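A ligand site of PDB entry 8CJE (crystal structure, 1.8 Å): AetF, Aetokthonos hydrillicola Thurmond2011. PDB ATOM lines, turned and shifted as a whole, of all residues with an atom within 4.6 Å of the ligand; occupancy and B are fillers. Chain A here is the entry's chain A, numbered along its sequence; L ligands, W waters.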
ATOM      1  N   ILE A  15      32.795   1.946  19.134  1.00  0.00           N
ATOM      2  CA  ILE A  15      31.457   2.300  19.584  1.00  0.00           C
ATOM      3  C   ILE A  15      31.068   3.646  18.974  1.00  0.00           C
ATOM      4  O   ILE A  15      31.665   4.682  19.301  1.00  0.00           O
ATOM      5  CB  ILE A  15      31.365   2.318  21.111  1.00  0.00           C
ATOM      6  CG1 ILE A  15      31.656   0.918  21.634  1.00  0.00           C
ATOM      7  CG2 ILE A  15      30.000   2.765  21.548  1.00  0.00           C
ATOM      8  CD1 ILE A  15      32.092   0.891  23.038  1.00  0.00           C
ATOM      9  N   GLY A  16      30.061   3.639  18.103  1.00  0.00           N
ATOM     10  CA  GLY A  16      29.615   4.851  17.450  1.00  0.00           C
ATOM     11  C   GLY A  16      30.156   4.922  16.042  1.00  0.00           C
ATOM     12  O   GLY A  16      31.376   4.914  15.852  1.00  0.00           O
ATOM     13  N   PHE A  17      29.276   4.980  15.035  1.00  0.00           N
ATOM     14  CA  PHE A  17      29.703   5.139  13.648  1.00  0.00           C
ATOM     15  C   PHE A  17      28.906   6.262  13.022  1.00  0.00           C
ATOM     16  O   PHE A  17      27.707   6.121  12.774  1.00  0.00           O
ATOM     17  CB  PHE A  17      29.517   3.852  12.845  1.00  0.00           C
ATOM     18  CG  PHE A  17      30.198   3.884  11.498  1.00  0.00           C
ATOM     19  CD1 PHE A  17      31.523   3.507  11.361  1.00  0.00           C
ATOM     20  CD2 PHE A  17      29.522   4.324  10.367  1.00  0.00           C
ATOM     21  CE1 PHE A  17      32.160   3.528  10.150  1.00  0.00           C
ATOM     22  CE2 PHE A  17      30.173   4.352   9.137  1.00  0.00           C
ATOM     23  CZ  PHE A  17      31.481   3.955   9.034  1.00  0.00           C
ATOM     24  N   GLY A  18      29.570   7.372  12.742  1.00  0.00           N
ATOM     25  CA  GLY A  18      28.951   8.460  12.018  1.00  0.00           C
ATOM     26  C   GLY A  18      29.884   9.043  10.991  1.00  0.00           C
ATOM     27  O   GLY A  18      29.855   8.665   9.823  1.00  0.00           O
ATOM     28  N   PHE A  19      30.724   9.953  11.427  1.00  0.00           N
ATOM     29  CA  PHE A  19      31.704  10.579  10.551  1.00  0.00           C
ATOM     30  C   PHE A  19      33.122  10.442  11.079  1.00  0.00           C
ATOM     31  O   PHE A  19      34.045  10.264  10.295  1.00  0.00           O
ATOM     32  CB  PHE A  19      31.329  12.057  10.343  1.00  0.00           C
ATOM     33  CG  PHE A  19      32.419  12.882   9.740  1.00  0.00           C
ATOM     34  CD1 PHE A  19      32.701  12.776   8.391  1.00  0.00           C
ATOM     35  CD2 PHE A  19      33.122  13.815  10.497  1.00  0.00           C
ATOM     36  CE1 PHE A  19      33.689  13.541   7.837  1.00  0.00           C
ATOM     37  CE2 PHE A  19      34.113  14.593   9.928  1.00  0.00           C
ATOM     38  CZ  PHE A  19      34.391  14.467   8.601  1.00  0.00           C
ATOM     39  N   SER A  20      33.300  10.513  12.401  1.00  0.00           N
ATOM     40  CA  SER A  20      34.629  10.465  12.983  1.00  0.00           C
ATOM     41  C   SER A  20      35.269   9.087  12.848  1.00  0.00           C
ATOM     42  O   SER A  20      36.493   8.975  12.739  1.00  0.00           O
ATOM     43  CB  SER A  20      34.547  10.864  14.447  1.00  0.00           C
ATOM     44  OG  SER A  20      34.060  12.188  14.574  1.00  0.00           O
ATOM     45  N   ILE A  38      29.784  -1.095  17.042  1.00  0.00           N
ATOM     46  CA  ILE A  38      28.453  -1.071  17.637  1.00  0.00           C
ATOM     47  C   ILE A  38      27.959   0.363  17.588  1.00  0.00           C
ATOM     48  O   ILE A  38      28.537   1.242  18.238  1.00  0.00           O
ATOM     49  CB  ILE A  38      28.434  -1.601  19.079  1.00  0.00           C
ATOM     50  CG1 ILE A  38      29.027  -3.010  19.145  1.00  0.00           C
ATOM     51  CG2 ILE A  38      27.018  -1.618  19.631  1.00  0.00           C
ATOM     52  CD1 ILE A  38      29.315  -3.464  20.524  1.00  0.00           C
ATOM     53  N   SER A  39      26.912   0.621  16.813  1.00  0.00           N
ATOM     54  CA  SER A  39      26.296   1.931  16.746  1.00  0.00           C
ATOM     55  C   SER A  39      24.776   1.782  16.823  1.00  0.00           C
ATOM     56  O   SER A  39      24.203   0.835  16.304  1.00  0.00           O
ATOM     57  CB  SER A  39      26.680   2.673  15.456  1.00  0.00           C
ATOM     58  OG  SER A  39      26.402   4.054  15.553  1.00  0.00           O
ATOM     59  N   ALA A  40      24.131   2.764  17.460  1.00  0.00           N
ATOM     60  CA  ALA A  40      22.720   2.665  17.735  1.00  0.00           C
ATOM     61  C   ALA A  40      21.879   2.838  16.466  1.00  0.00           C
ATOM     62  O   ALA A  40      22.199   3.666  15.615  1.00  0.00           O
ATOM     63  CB  ALA A  40      22.311   3.696  18.778  1.00  0.00           C
ATOM     64  N   GLY A  43      20.719   6.664  15.207  1.00  0.00           N
ATOM     65  CA  GLY A  43      21.376   7.495  14.228  1.00  0.00           C
ATOM     66  C   GLY A  43      21.825   8.821  14.811  1.00  0.00           C
ATOM     67  O   GLY A  43      21.822   9.038  16.027  1.00  0.00           O
ATOM     68  N   SER A  44      22.223   9.717  13.930  1.00  0.00           N
ATOM     69  CA  SER A  44      22.827  10.980  14.311  1.00  0.00           C
ATOM     70  C   SER A  44      21.865  12.142  14.115  1.00  0.00           C
ATOM     71  O   SER A  44      20.754  12.009  13.595  1.00  0.00           O
ATOM     72  CB  SER A  44      24.108  11.195  13.516  1.00  0.00           C
ATOM     73  OG  SER A  44      23.810  11.381  12.155  1.00  0.00           O
ATOM     74  N   VAL A  45      22.333  13.331  14.510  1.00  0.00           N
ATOM     75  CA  VAL A  45      21.597  14.564  14.244  1.00  0.00           C
ATOM     76  C   VAL A  45      21.392  14.731  12.755  1.00  0.00           C
ATOM     77  O   VAL A  45      20.407  15.331  12.314  1.00  0.00           O
ATOM     78  CB  VAL A  45      22.336  15.769  14.836  1.00  0.00           C
ATOM     79  CG1 VAL A  45      23.774  15.801  14.331  1.00  0.00           C
ATOM     80  CG2 VAL A  45      21.626  17.049  14.480  1.00  0.00           C
ATOM     81  N   TRP A  46      22.353  14.262  11.947  1.00  0.00           N
ATOM     82  CA  TRP A  46      22.198  14.344  10.512  1.00  0.00           C
ATOM     83  C   TRP A  46      21.041  13.477  10.041  1.00  0.00           C
ATOM     84  O   TRP A  46      20.305  13.865   9.131  1.00  0.00           O
ATOM     85  CB  TRP A  46      23.506  13.959   9.827  1.00  0.00           C
ATOM     86  CG  TRP A  46      24.652  14.791  10.304  1.00  0.00           C
ATOM     87  CD1 TRP A  46      25.554  14.476  11.263  1.00  0.00           C
ATOM     88  CD2 TRP A  46      24.977  16.098   9.839  1.00  0.00           C
ATOM     89  NE1 TRP A  46      26.444  15.516  11.425  1.00  0.00           N
ATOM     90  CE2 TRP A  46      26.100  16.531  10.571  1.00  0.00           C
ATOM     91  CE3 TRP A  46      24.434  16.962   8.881  1.00  0.00           C
ATOM     92  CZ2 TRP A  46      26.693  17.764  10.369  1.00  0.00           C
ATOM     93  CZ3 TRP A  46      25.015  18.195   8.692  1.00  0.00           C
ATOM     94  CH2 TRP A  46      26.136  18.586   9.424  1.00  0.00           C
ATOM     95  N   PHE A  57      20.971  23.508   4.659  1.00  0.00           N
ATOM     96  CA  PHE A  57      21.988  24.484   5.024  1.00  0.00           C
ATOM     97  C   PHE A  57      23.366  24.057   4.510  1.00  0.00           C
ATOM     98  O   PHE A  57      23.507  23.066   3.793  1.00  0.00           O
ATOM     99  CB  PHE A  57      21.965  24.761   6.536  1.00  0.00           C
ATOM    100  CG  PHE A  57      22.235  23.557   7.389  1.00  0.00           C
ATOM    101  CD1 PHE A  57      21.236  22.632   7.629  1.00  0.00           C
ATOM    102  CD2 PHE A  57      23.469  23.369   7.972  1.00  0.00           C
ATOM    103  CE1 PHE A  57      21.470  21.520   8.409  1.00  0.00           C
ATOM    104  CE2 PHE A  57      23.711  22.264   8.761  1.00  0.00           C
ATOM    105  CZ  PHE A  57      22.697  21.332   8.976  1.00  0.00           C
ATOM    106  N   LEU A  59      27.897  23.909   5.175  1.00  0.00           N
ATOM    107  CA  LEU A  59      28.962  23.753   6.152  1.00  0.00           C
ATOM    108  C   LEU A  59      29.633  25.104   6.393  1.00  0.00           C
ATOM    109  O   LEU A  59      29.688  25.952   5.496  1.00  0.00           O
ATOM    110  CB  LEU A  59      30.013  22.749   5.686  1.00  0.00           C
ATOM    111  CG  LEU A  59      29.596  21.312   5.369  1.00  0.00           C
ATOM    112  CD1 LEU A  59      30.817  20.422   5.289  1.00  0.00           C
ATOM    113  CD2 LEU A  59      28.608  20.788   6.371  1.00  0.00           C
ATOM    114  N   VAL A  60      30.159  25.291   7.600  1.00  0.00           N
ATOM    115  CA  VAL A  60      30.908  26.500   7.900  1.00  0.00           C
ATOM    116  C   VAL A  60      32.380  26.202   7.687  1.00  0.00           C
ATOM    117  O   VAL A  60      33.246  26.998   8.072  1.00  0.00           O
ATOM    118  CB  VAL A  60      30.654  27.051   9.324  1.00  0.00           C
ATOM    119  CG1 VAL A  60      29.202  27.482   9.502  1.00  0.00           C
ATOM    120  CG2 VAL A  60      31.025  26.052  10.384  1.00  0.00           C
ATOM    121  N   SER A  61      32.670  25.067   7.084  1.00  0.00           N
ATOM    122  CA  SER A  61      34.023  24.575   6.883  1.00  0.00           C
ATOM    123  C   SER A  61      34.217  24.209   5.417  1.00  0.00           C
ATOM    124  O   SER A  61      33.302  23.686   4.766  1.00  0.00           O
ATOM    125  CB  SER A  61      34.308  23.378   7.760  1.00  0.00           C
ATOM    126  OG  SER A  61      33.409  22.344   7.473  1.00  0.00           O
ATOM    127  N   PHE A  87      27.333  16.830   2.861  1.00  0.00           N
ATOM    128  CA  PHE A  87      28.054  16.268   4.009  1.00  0.00           C
ATOM    129  C   PHE A  87      27.441  14.947   4.431  1.00  0.00           C
ATOM    130  O   PHE A  87      28.150  13.947   4.595  1.00  0.00           O
ATOM    131  CB  PHE A  87      28.030  17.269   5.170  1.00  0.00           C
ATOM    132  CG  PHE A  87      29.043  16.989   6.255  1.00  0.00           C
ATOM    133  CD1 PHE A  87      30.369  16.772   5.950  1.00  0.00           C
ATOM    134  CD2 PHE A  87      28.660  16.977   7.581  1.00  0.00           C
ATOM    135  CE1 PHE A  87      31.286  16.529   6.954  1.00  0.00           C
ATOM    136  CE2 PHE A  87      29.577  16.748   8.584  1.00  0.00           C
ATOM    137  CZ  PHE A  87      30.886  16.516   8.263  1.00  0.00           C
ATOM    138  N   HIS A  91      28.531  10.788   4.586  1.00  0.00           N
ATOM    139  CA  HIS A  91      28.387   9.925   5.762  1.00  0.00           C
ATOM    140  C   HIS A  91      27.717   8.608   5.399  1.00  0.00           C
ATOM    141  O   HIS A  91      28.195   7.539   5.775  1.00  0.00           O
ATOM    142  CB  HIS A  91      27.567  10.628   6.841  1.00  0.00           C
ATOM    143  CG  HIS A  91      28.173  11.900   7.330  1.00  0.00           C
ATOM    144  ND1 HIS A  91      27.496  12.744   8.194  1.00  0.00           N
ATOM    145  CD2 HIS A  91      29.387  12.444   7.142  1.00  0.00           C
ATOM    146  CE1 HIS A  91      28.263  13.775   8.479  1.00  0.00           C
ATOM    147  NE2 HIS A  91      29.422  13.621   7.865  1.00  0.00           N
ATOM    148  N   ASP A 105      23.174  -1.694  18.020  1.00  0.00           N
ATOM    149  CA  ASP A 105      22.827  -1.770  19.419  1.00  0.00           C
ATOM    150  C   ASP A 105      23.354  -0.501  20.074  1.00  0.00           C
ATOM    151  O   ASP A 105      24.097   0.262  19.470  1.00  0.00           O
ATOM    152  CB  ASP A 105      23.386  -3.049  20.057  1.00  0.00           C
ATOM    153  CG  ASP A 105      22.585  -3.512  21.270  1.00  0.00           C
ATOM    154  OD1 ASP A 105      21.731  -2.760  21.796  1.00  0.00           O
ATOM    155  OD2 ASP A 105      22.801  -4.665  21.681  1.00  0.00           O
ATOM    156  N   PHE A 106      22.987  -0.310  21.334  1.00  0.00           N
ATOM    157  CA  PHE A 106      23.339   0.866  22.104  1.00  0.00           C
ATOM    158  C   PHE A 106      24.166   0.437  23.304  1.00  0.00           C
ATOM    159  O   PHE A 106      23.712  -0.381  24.110  1.00  0.00           O
ATOM    160  CB  PHE A 106      22.089   1.621  22.569  1.00  0.00           C
ATOM    161  CG  PHE A 106      22.406   2.883  23.318  1.00  0.00           C
ATOM    162  CD1 PHE A 106      22.802   4.023  22.660  1.00  0.00           C
ATOM    163  CD2 PHE A 106      22.309   2.913  24.700  1.00  0.00           C
ATOM    164  CE1 PHE A 106      23.095   5.178  23.356  1.00  0.00           C
ATOM    165  CE2 PHE A 106      22.622   4.068  25.399  1.00  0.00           C
ATOM    166  CZ  PHE A 106      23.013   5.194  24.713  1.00  0.00           C
ATOM    167  N   VAL A 107      25.369   0.986  23.415  1.00  0.00           N
ATOM    168  CA  VAL A 107      26.267   0.617  24.504  1.00  0.00           C
ATOM    169  C   VAL A 107      25.897   1.403  25.752  1.00  0.00           C
ATOM    170  O   VAL A 107      25.751   2.630  25.710  1.00  0.00           O
ATOM    171  CB  VAL A 107      27.733   0.869  24.107  1.00  0.00           C
ATOM    172  CG1 VAL A 107      28.647   0.664  25.302  1.00  0.00           C
ATOM    173  CG2 VAL A 107      28.109  -0.070  22.977  1.00  0.00           C
ATOM    174  N   ALA A 135      33.566   6.899  19.601  1.00  0.00           N
ATOM    175  CA  ALA A 135      33.373   7.965  18.643  1.00  0.00           C
ATOM    176  C   ALA A 135      31.881   8.287  18.565  1.00  0.00           C
ATOM    177  O   ALA A 135      31.273   8.267  17.505  1.00  0.00           O
ATOM    178  CB  ALA A 135      33.947   7.590  17.271  1.00  0.00           C
ATOM    179  N   THR A 136      31.296   8.645  19.706  1.00  0.00           N
ATOM    180  CA  THR A 136      29.849   8.758  19.869  1.00  0.00           C
ATOM    181  C   THR A 136      29.303  10.192  19.711  1.00  0.00           C
ATOM    182  O   THR A 136      28.077  10.360  19.775  1.00  0.00           O
ATOM    183  CB  THR A 136      29.415   8.209  21.240  1.00  0.00           C
ATOM    184  OG1 THR A 136      30.147   8.856  22.259  1.00  0.00           O
ATOM    185  CG2 THR A 136      29.657   6.726  21.333  1.00  0.00           C
ATOM    186  N   GLY A 137      30.154  11.199  19.508  1.00  0.00           N
ATOM    187  CA  GLY A 137      29.694  12.559  19.309  1.00  0.00           C
ATOM    188  C   GLY A 137      29.316  13.282  20.593  1.00  0.00           C
ATOM    189  O   GLY A 137      29.703  12.892  21.701  1.00  0.00           O
ATOM    190  N   ARG A 140      23.616  18.243  22.252  1.00  0.00           N
ATOM    191  CA  ARG A 140      23.282  19.660  22.274  1.00  0.00           C
ATOM    192  C   ARG A 140      21.765  19.757  22.253  1.00  0.00           C
ATOM    193  O   ARG A 140      21.133  19.181  21.366  1.00  0.00           O
ATOM    194  CB  ARG A 140      23.864  20.390  21.069  1.00  0.00           C
ATOM    195  CG  ARG A 140      25.324  20.120  20.752  1.00  0.00           C
ATOM    196  CD  ARG A 140      25.397  19.644  19.324  1.00  0.00           C
ATOM    197  NE  ARG A 140      26.726  19.226  18.866  1.00  0.00           N
ATOM    198  CZ  ARG A 140      26.952  18.155  18.115  1.00  0.00           C
ATOM    199  NH1 ARG A 140      25.981  17.321  17.798  1.00  0.00           N
ATOM    200  NH2 ARG A 140      28.181  17.924  17.665  1.00  0.00           N
ATOM    201  N   ASN A 143      20.280  21.100  19.006  1.00  0.00           N
ATOM    202  CA  ASN A 143      19.901  20.280  17.858  1.00  0.00           C
ATOM    203  C   ASN A 143      18.400  20.051  17.818  1.00  0.00           C
ATOM    204  O   ASN A 143      17.774  20.229  16.766  1.00  0.00           O
ATOM    205  CB  ASN A 143      20.636  18.945  17.882  1.00  0.00           C
ATOM    206  CG  ASN A 143      22.126  19.094  17.800  1.00  0.00           C
ATOM    207  OD1 ASN A 143      22.624  20.165  17.478  1.00  0.00           O
ATOM    208  ND2 ASN A 143      22.852  18.025  18.083  1.00  0.00           N
ATOM    209  N   LEU A 146      16.601  23.044  16.494  1.00  0.00           N
ATOM    210  CA  LEU A 146      16.604  23.249  15.041  1.00  0.00           C
ATOM    211  C   LEU A 146      15.657  22.295  14.342  1.00  0.00           C
ATOM    212  O   LEU A 146      15.129  22.612  13.276  1.00  0.00           O
ATOM    213  CB  LEU A 146      18.000  23.054  14.460  1.00  0.00           C
ATOM    214  CG  LEU A 146      19.139  23.929  14.921  1.00  0.00           C
ATOM    215  CD1 LEU A 146      20.444  23.273  14.564  1.00  0.00           C
ATOM    216  CD2 LEU A 146      19.019  25.245  14.221  1.00  0.00           C
ATOM    217  N   SER A 166      25.228  27.707  15.528  1.00  0.00           N
ATOM    218  CA  SER A 166      23.829  27.284  15.459  1.00  0.00           C
ATOM    219  C   SER A 166      22.888  28.471  15.603  1.00  0.00           C
ATOM    220  O   SER A 166      21.848  28.539  14.941  1.00  0.00           O
ATOM    221  CB  SER A 166      23.506  26.247  16.528  1.00  0.00           C
ATOM    222  OG  SER A 166      23.860  24.930  16.113  1.00  0.00           O
ATOM    223  N   ARG A 340      28.771  12.286  24.473  1.00  0.00           N
ATOM    224  CA  ARG A 340      27.865  11.160  24.676  1.00  0.00           C
ATOM    225  C   ARG A 340      28.655   9.935  25.102  1.00  0.00           C
ATOM    226  O   ARG A 340      28.867   9.006  24.331  1.00  0.00           O
ATOM    227  CB  ARG A 340      27.105  10.843  23.395  1.00  0.00           C
ATOM    228  CG  ARG A 340      26.089  11.840  22.898  1.00  0.00           C
ATOM    229  CD  ARG A 340      25.315  11.172  21.765  1.00  0.00           C
ATOM    230  NE  ARG A 340      24.698  12.101  20.829  1.00  0.00           N
ATOM    231  CZ  ARG A 340      25.004  12.159  19.546  1.00  0.00           C
ATOM    232  NH1 ARG A 340      25.926  11.362  19.032  1.00  0.00           N
ATOM    233  NH2 ARG A 340      24.390  13.041  18.762  1.00  0.00           N
ATOM    234  N   GLY A 375      36.944  12.109  17.895  1.00  0.00           N
ATOM    235  CA  GLY A 375      35.921  13.073  17.549  1.00  0.00           C
ATOM    236  C   GLY A 375      35.576  14.067  18.625  1.00  0.00           C
ATOM    237  O   GLY A 375      34.643  14.839  18.434  1.00  0.00           O
ATOM    238  N   GLY A 382      37.873  25.388  10.024  1.00  0.00           N
ATOM    239  CA  GLY A 382      37.809  24.266   9.124  1.00  0.00           C
ATOM    240  C   GLY A 382      36.991  23.129   9.700  1.00  0.00           C
ATOM    241  O   GLY A 382      36.440  23.202  10.781  1.00  0.00           O
ATOM    242  N   GLY A 383      36.988  22.029   8.975  1.00  0.00           N
ATOM    243  CA  GLY A 383      36.127  20.926   9.335  1.00  0.00           C
ATOM    244  C   GLY A 383      36.719  20.005  10.360  1.00  0.00           C
ATOM    245  O   GLY A 383      37.904  20.027  10.672  1.00  0.00           O
ATOM    246  N   LEU A 384      35.850  19.159  10.915  1.00  0.00           N
ATOM    247  CA  LEU A 384      36.290  18.150  11.865  1.00  0.00           C
ATOM    248  C   LEU A 384      37.171  17.098  11.206  1.00  0.00           C
ATOM    249  O   LEU A 384      38.014  16.505  11.880  1.00  0.00           O
ATOM    250  CB  LEU A 384      35.082  17.485  12.530  1.00  0.00           C
ATOM    251  CG  LEU A 384      35.335  16.383  13.550  1.00  0.00           C
ATOM    252  CD1 LEU A 384      36.012  16.962  14.761  1.00  0.00           C
ATOM    253  CD2 LEU A 384      34.055  15.680  13.924  1.00  0.00           C
HETATM  254  P1  LIG L   1      27.913  11.471  15.203  1.00  0.00           P
HETATM  255  O1  LIG L   1      27.805  11.800  13.764  1.00  0.00           O
HETATM  256  O2  LIG L   1      26.827  12.058  16.045  1.00  0.00           O
HETATM  257  O3  LIG L   1      28.000   9.977  15.255  1.00  0.00           O
HETATM  258  C1  LIG L   1      27.959   9.268  16.503  1.00  0.00           C
HETATM  259  C2  LIG L   1      27.124   8.028  16.282  1.00  0.00           C
HETATM  260  O4  LIG L   1      27.304   7.127  17.400  1.00  0.00           O
HETATM  261  C3  LIG L   1      25.622   8.250  16.133  1.00  0.00           C
HETATM  262  O5  LIG L   1      25.102   7.443  15.097  1.00  0.00           O
HETATM  263  C4  LIG L   1      25.081   7.832  17.497  1.00  0.00           C
HETATM  264  O6  LIG L   1      23.740   7.344  17.432  1.00  0.00           O
HETATM  265  C5  LIG L   1      26.034   6.709  17.871  1.00  0.00           C
HETATM  266  N1  LIG L   1      26.134   6.451  19.307  1.00  0.00           N
HETATM  267  C6  LIG L   1      26.247   7.376  20.306  1.00  0.00           C
HETATM  268  N2  LIG L   1      26.311   6.868  21.504  1.00  0.00           N
HETATM  269  C7  LIG L   1      26.245   5.501  21.283  1.00  0.00           C
HETATM  270  C8  LIG L   1      26.269   4.403  22.162  1.00  0.00           C
HETATM  271  N3  LIG L   1      26.367   4.505  23.483  1.00  0.00           N
HETATM  272  N4  LIG L   1      26.182   3.166  21.611  1.00  0.00           N
HETATM  273  C9  LIG L   1      26.082   3.057  20.297  1.00  0.00           C
HETATM  274  N5  LIG L   1      26.044   4.021  19.367  1.00  0.00           N
HETATM  275  C10 LIG L   1      26.137   5.229  19.934  1.00  0.00           C
HETATM  276  N6  LIG L   1      31.492  19.752  11.427  1.00  0.00           N
HETATM  277  C11 LIG L   1      32.241  20.254  10.398  1.00  0.00           C
HETATM  278  O7  LIG L   1      33.392  19.887  10.210  1.00  0.00           O
HETATM  279  N7  LIG L   1      31.698  21.204   9.568  1.00  0.00           N
HETATM  280  C12 LIG L   1      30.417  21.714   9.645  1.00  0.00           C
HETATM  281  O8  LIG L   1      30.019  22.562   8.842  1.00  0.00           O
HETATM  282  C13 LIG L   1      29.628  21.171  10.725  1.00  0.00           C
HETATM  283  N8  LIG L   1      28.396  21.603  10.862  1.00  0.00           N
HETATM  284  C14 LIG L   1      27.644  21.086  11.905  1.00  0.00           C
HETATM  285  C15 LIG L   1      26.326  21.528  12.077  1.00  0.00           C
HETATM  286  C16 LIG L   1      25.526  21.034  13.104  1.00  0.00           C
HETATM  287  C17 LIG L   1      24.119  21.541  13.267  1.00  0.00           C
HETATM  288  C18 LIG L   1      26.050  20.071  13.988  1.00  0.00           C
HETATM  289  C19 LIG L   1      25.230  19.516  15.121  1.00  0.00           C
HETATM  290  C20 LIG L   1      27.368  19.651  13.823  1.00  0.00           C
HETATM  291  C21 LIG L   1      28.156  20.138  12.801  1.00  0.00           C
HETATM  292  N9  LIG L   1      29.481  19.682  12.587  1.00  0.00           N
HETATM  293  C22 LIG L   1      30.248  20.198  11.576  1.00  0.00           C
HETATM  294  C23 LIG L   1      30.090  18.724  13.508  1.00  0.00           C
HETATM  295  C24 LIG L   1      29.437  17.354  13.451  1.00  0.00           C
HETATM  296  O9  LIG L   1      28.949  17.004  14.751  1.00  0.00           O
HETATM  297  C25 LIG L   1      30.469  16.350  12.981  1.00  0.00           C
HETATM  298  O10 LIG L   1      30.962  16.799  11.723  1.00  0.00           O
HETATM  299  C26 LIG L   1      29.886  14.950  12.922  1.00  0.00           C
HETATM  300  O11 LIG L   1      28.479  14.978  12.728  1.00  0.00           O
HETATM  301  C27 LIG L   1      30.170  14.254  14.233  1.00  0.00           C
HETATM  302  O12 LIG L   1      30.593  12.923  13.945  1.00  0.00           O
HETATM  303  P2  LIG L   1      30.699  11.861  15.061  1.00  0.00           P
HETATM  304  O13 LIG L   1      30.782  10.525  14.333  1.00  0.00           O
HETATM  305  O14 LIG L   1      31.754  12.320  15.945  1.00  0.00           O
HETATM  306  O15 LIG L   1      29.297  11.973  15.785  1.00  0.00           O
HETATM  307  O   HOH W   1      25.676   8.136  12.821  1.00  0.00           O
HETATM  308  O   HOH W   2      32.732  11.385  18.135  1.00  0.00           O
HETATM  309  O   HOH W   3      31.891  14.901  17.103  1.00  0.00           O
HETATM  310  O   HOH W   4      26.277   7.325  25.042  1.00  0.00           O
HETATM  311  O   HOH W   5      27.080  23.445   9.170  1.00  0.00           O
HETATM  312  O   HOH W   6      34.480  17.515   8.693  1.00  0.00           O
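The backbone carbonyl oxygen (O) of Val 107 lies within hydrogen-bond range of a nitrogen (N3) of the ligand.
An oxygen (O14) of the ligand lies within hydrogen-bond range of the side-chain hydroxyl (OG) of Ser 20 (2.7 Å).
N of Val 60 sits at hydrogen-bond distance from O8 of the ligand (3.0 Å).
The backbone NH of Ser 20 sits at hydrogen-bond distance from an oxygen (O13) of the ligand (3.2 Å).
The indole nitrogen (NE1) of Trp 46 lies within hydrogen-bond range of an oxygen (O11) of the ligand, at 2.5 Å.
O9 of the ligand is in hydrogen-bond range of NH2 of Arg 140 (3.2 Å).
The backbone carbonyl oxygen (O) of Gly 43 is in hydrogen-bond range of an oxygen (O6) of the ligand (2.9 Å).
The backbone NH (N) of Ala 40 sits at hydrogen-bond distance from a nitrogen (N5) of the ligand, at 3.0 Å.
N of Val 107 is in hydrogen-bond range of N4 of the ligand, 2.9 Å away.
The guanidinium group (NH1) of Arg 340 is in salt-bridge range of an oxygen (O2) of the ligand.
The backbone NH (N) of Leu 384 is in hydrogen-bond range of an oxygen (O7) of the ligand (2.7 Å).
The backbone NH of Phe 19 sits at hydrogen-bond distance from an oxygen (O13) of the ligand.
OG of Ser 61 lies within hydrogen-bond range of N7 of the ligand (2.9 Å).
Water W1 lies within hydrogen-bond range of O5 of the ligand (2.4 Å) and O of Phe 17 (2.9 Å).
Water W2 lies within hydrogen-bond range of O14 of the ligand, N of Gly 137, N of Thr 136 and O of Ala 135.
Water W3 bridges an oxygen (O14) of the ligand and the backbone carbonyl oxygen of Gly 375.
Water W6 bridges an oxygen (O7) of the ligand (3.0 Å) and the backbone NH (N) of Leu 384 (3.1 Å).
Water W4 bridges O of Arg 340 (3.2 Å) and N3 of the ligand (3.2 Å).
CG2 of Ile 15 touches N4 of the ligand, at 3.8 Å.
Gly 16 touches the ligand.
Phe 17 touches the ligand.
CA of Gly 18 touches O13 of the ligand, at 3.6 Å.
Ile 38 touches the ligand (O to C9, 3.7 Å).
Ser 39 touches the ligand.
CB of Ser 44 touches O1 of the ligand, 3.8 Å away.
Leu 59 touches the ligand.
Phe 87 touches the ligand (CE2 to O10, 3.4 Å).
Asp 105 touches the ligand.
Phe 106 touches the ligand (CE1 to N3, 3.3 Å).
Ala 135 touches the ligand.
CG2 of Thr 136 touches N2 of the ligand, at 3.4 Å.
Gly 137 touches the ligand (CA to O15, 3.6 Å).
OD1 of Asn 143 touches C19 of the ligand (3.6 Å).
Gly 383 touches the ligand.
Hydrophobic or aromatic side chains that line the ligand: Ile 15, Phe 19, Ala 40, Trp 46, Leu 59, Val 60, Phe 87, Phe 106, Val 107 and Leu 384.
The nearest printed residue that does not touch the ligand is Val 45 (4.1 Å).
N of Arg 340 sits at hydrogen-bond distance from O of Gly 137, 3.0 Å away.
The backbone carbonyl oxygen (O) of Ser 39 sits at hydrogen-bond distance from the backbone NH (N) of Asp 105 (3.2 Å).
OG1 of Thr 136 is in hydrogen-bond range of O of Arg 340, at 2.4 Å.
The backbone NH (N) of Ala 135 is in hydrogen-bond range of the backbone carbonyl oxygen (O) of Ile 15 (2.9 Å).
NH1 of Arg 140 lies close to ND2 of Asn 143 (3.2 Å).
The backbone NH (N) of Phe 17 sits at hydrogen-bond distance from the side-chain hydroxyl (OG) of Ser 39, 3.1 Å away.
The backbone NH (N) of Gly 16 lies within hydrogen-bond range of the backbone carbonyl oxygen (O) of Ile 38 (2.8 Å).
O of Asp 105 is in hydrogen-bond range of N of Ala 40, 3.2 Å away.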
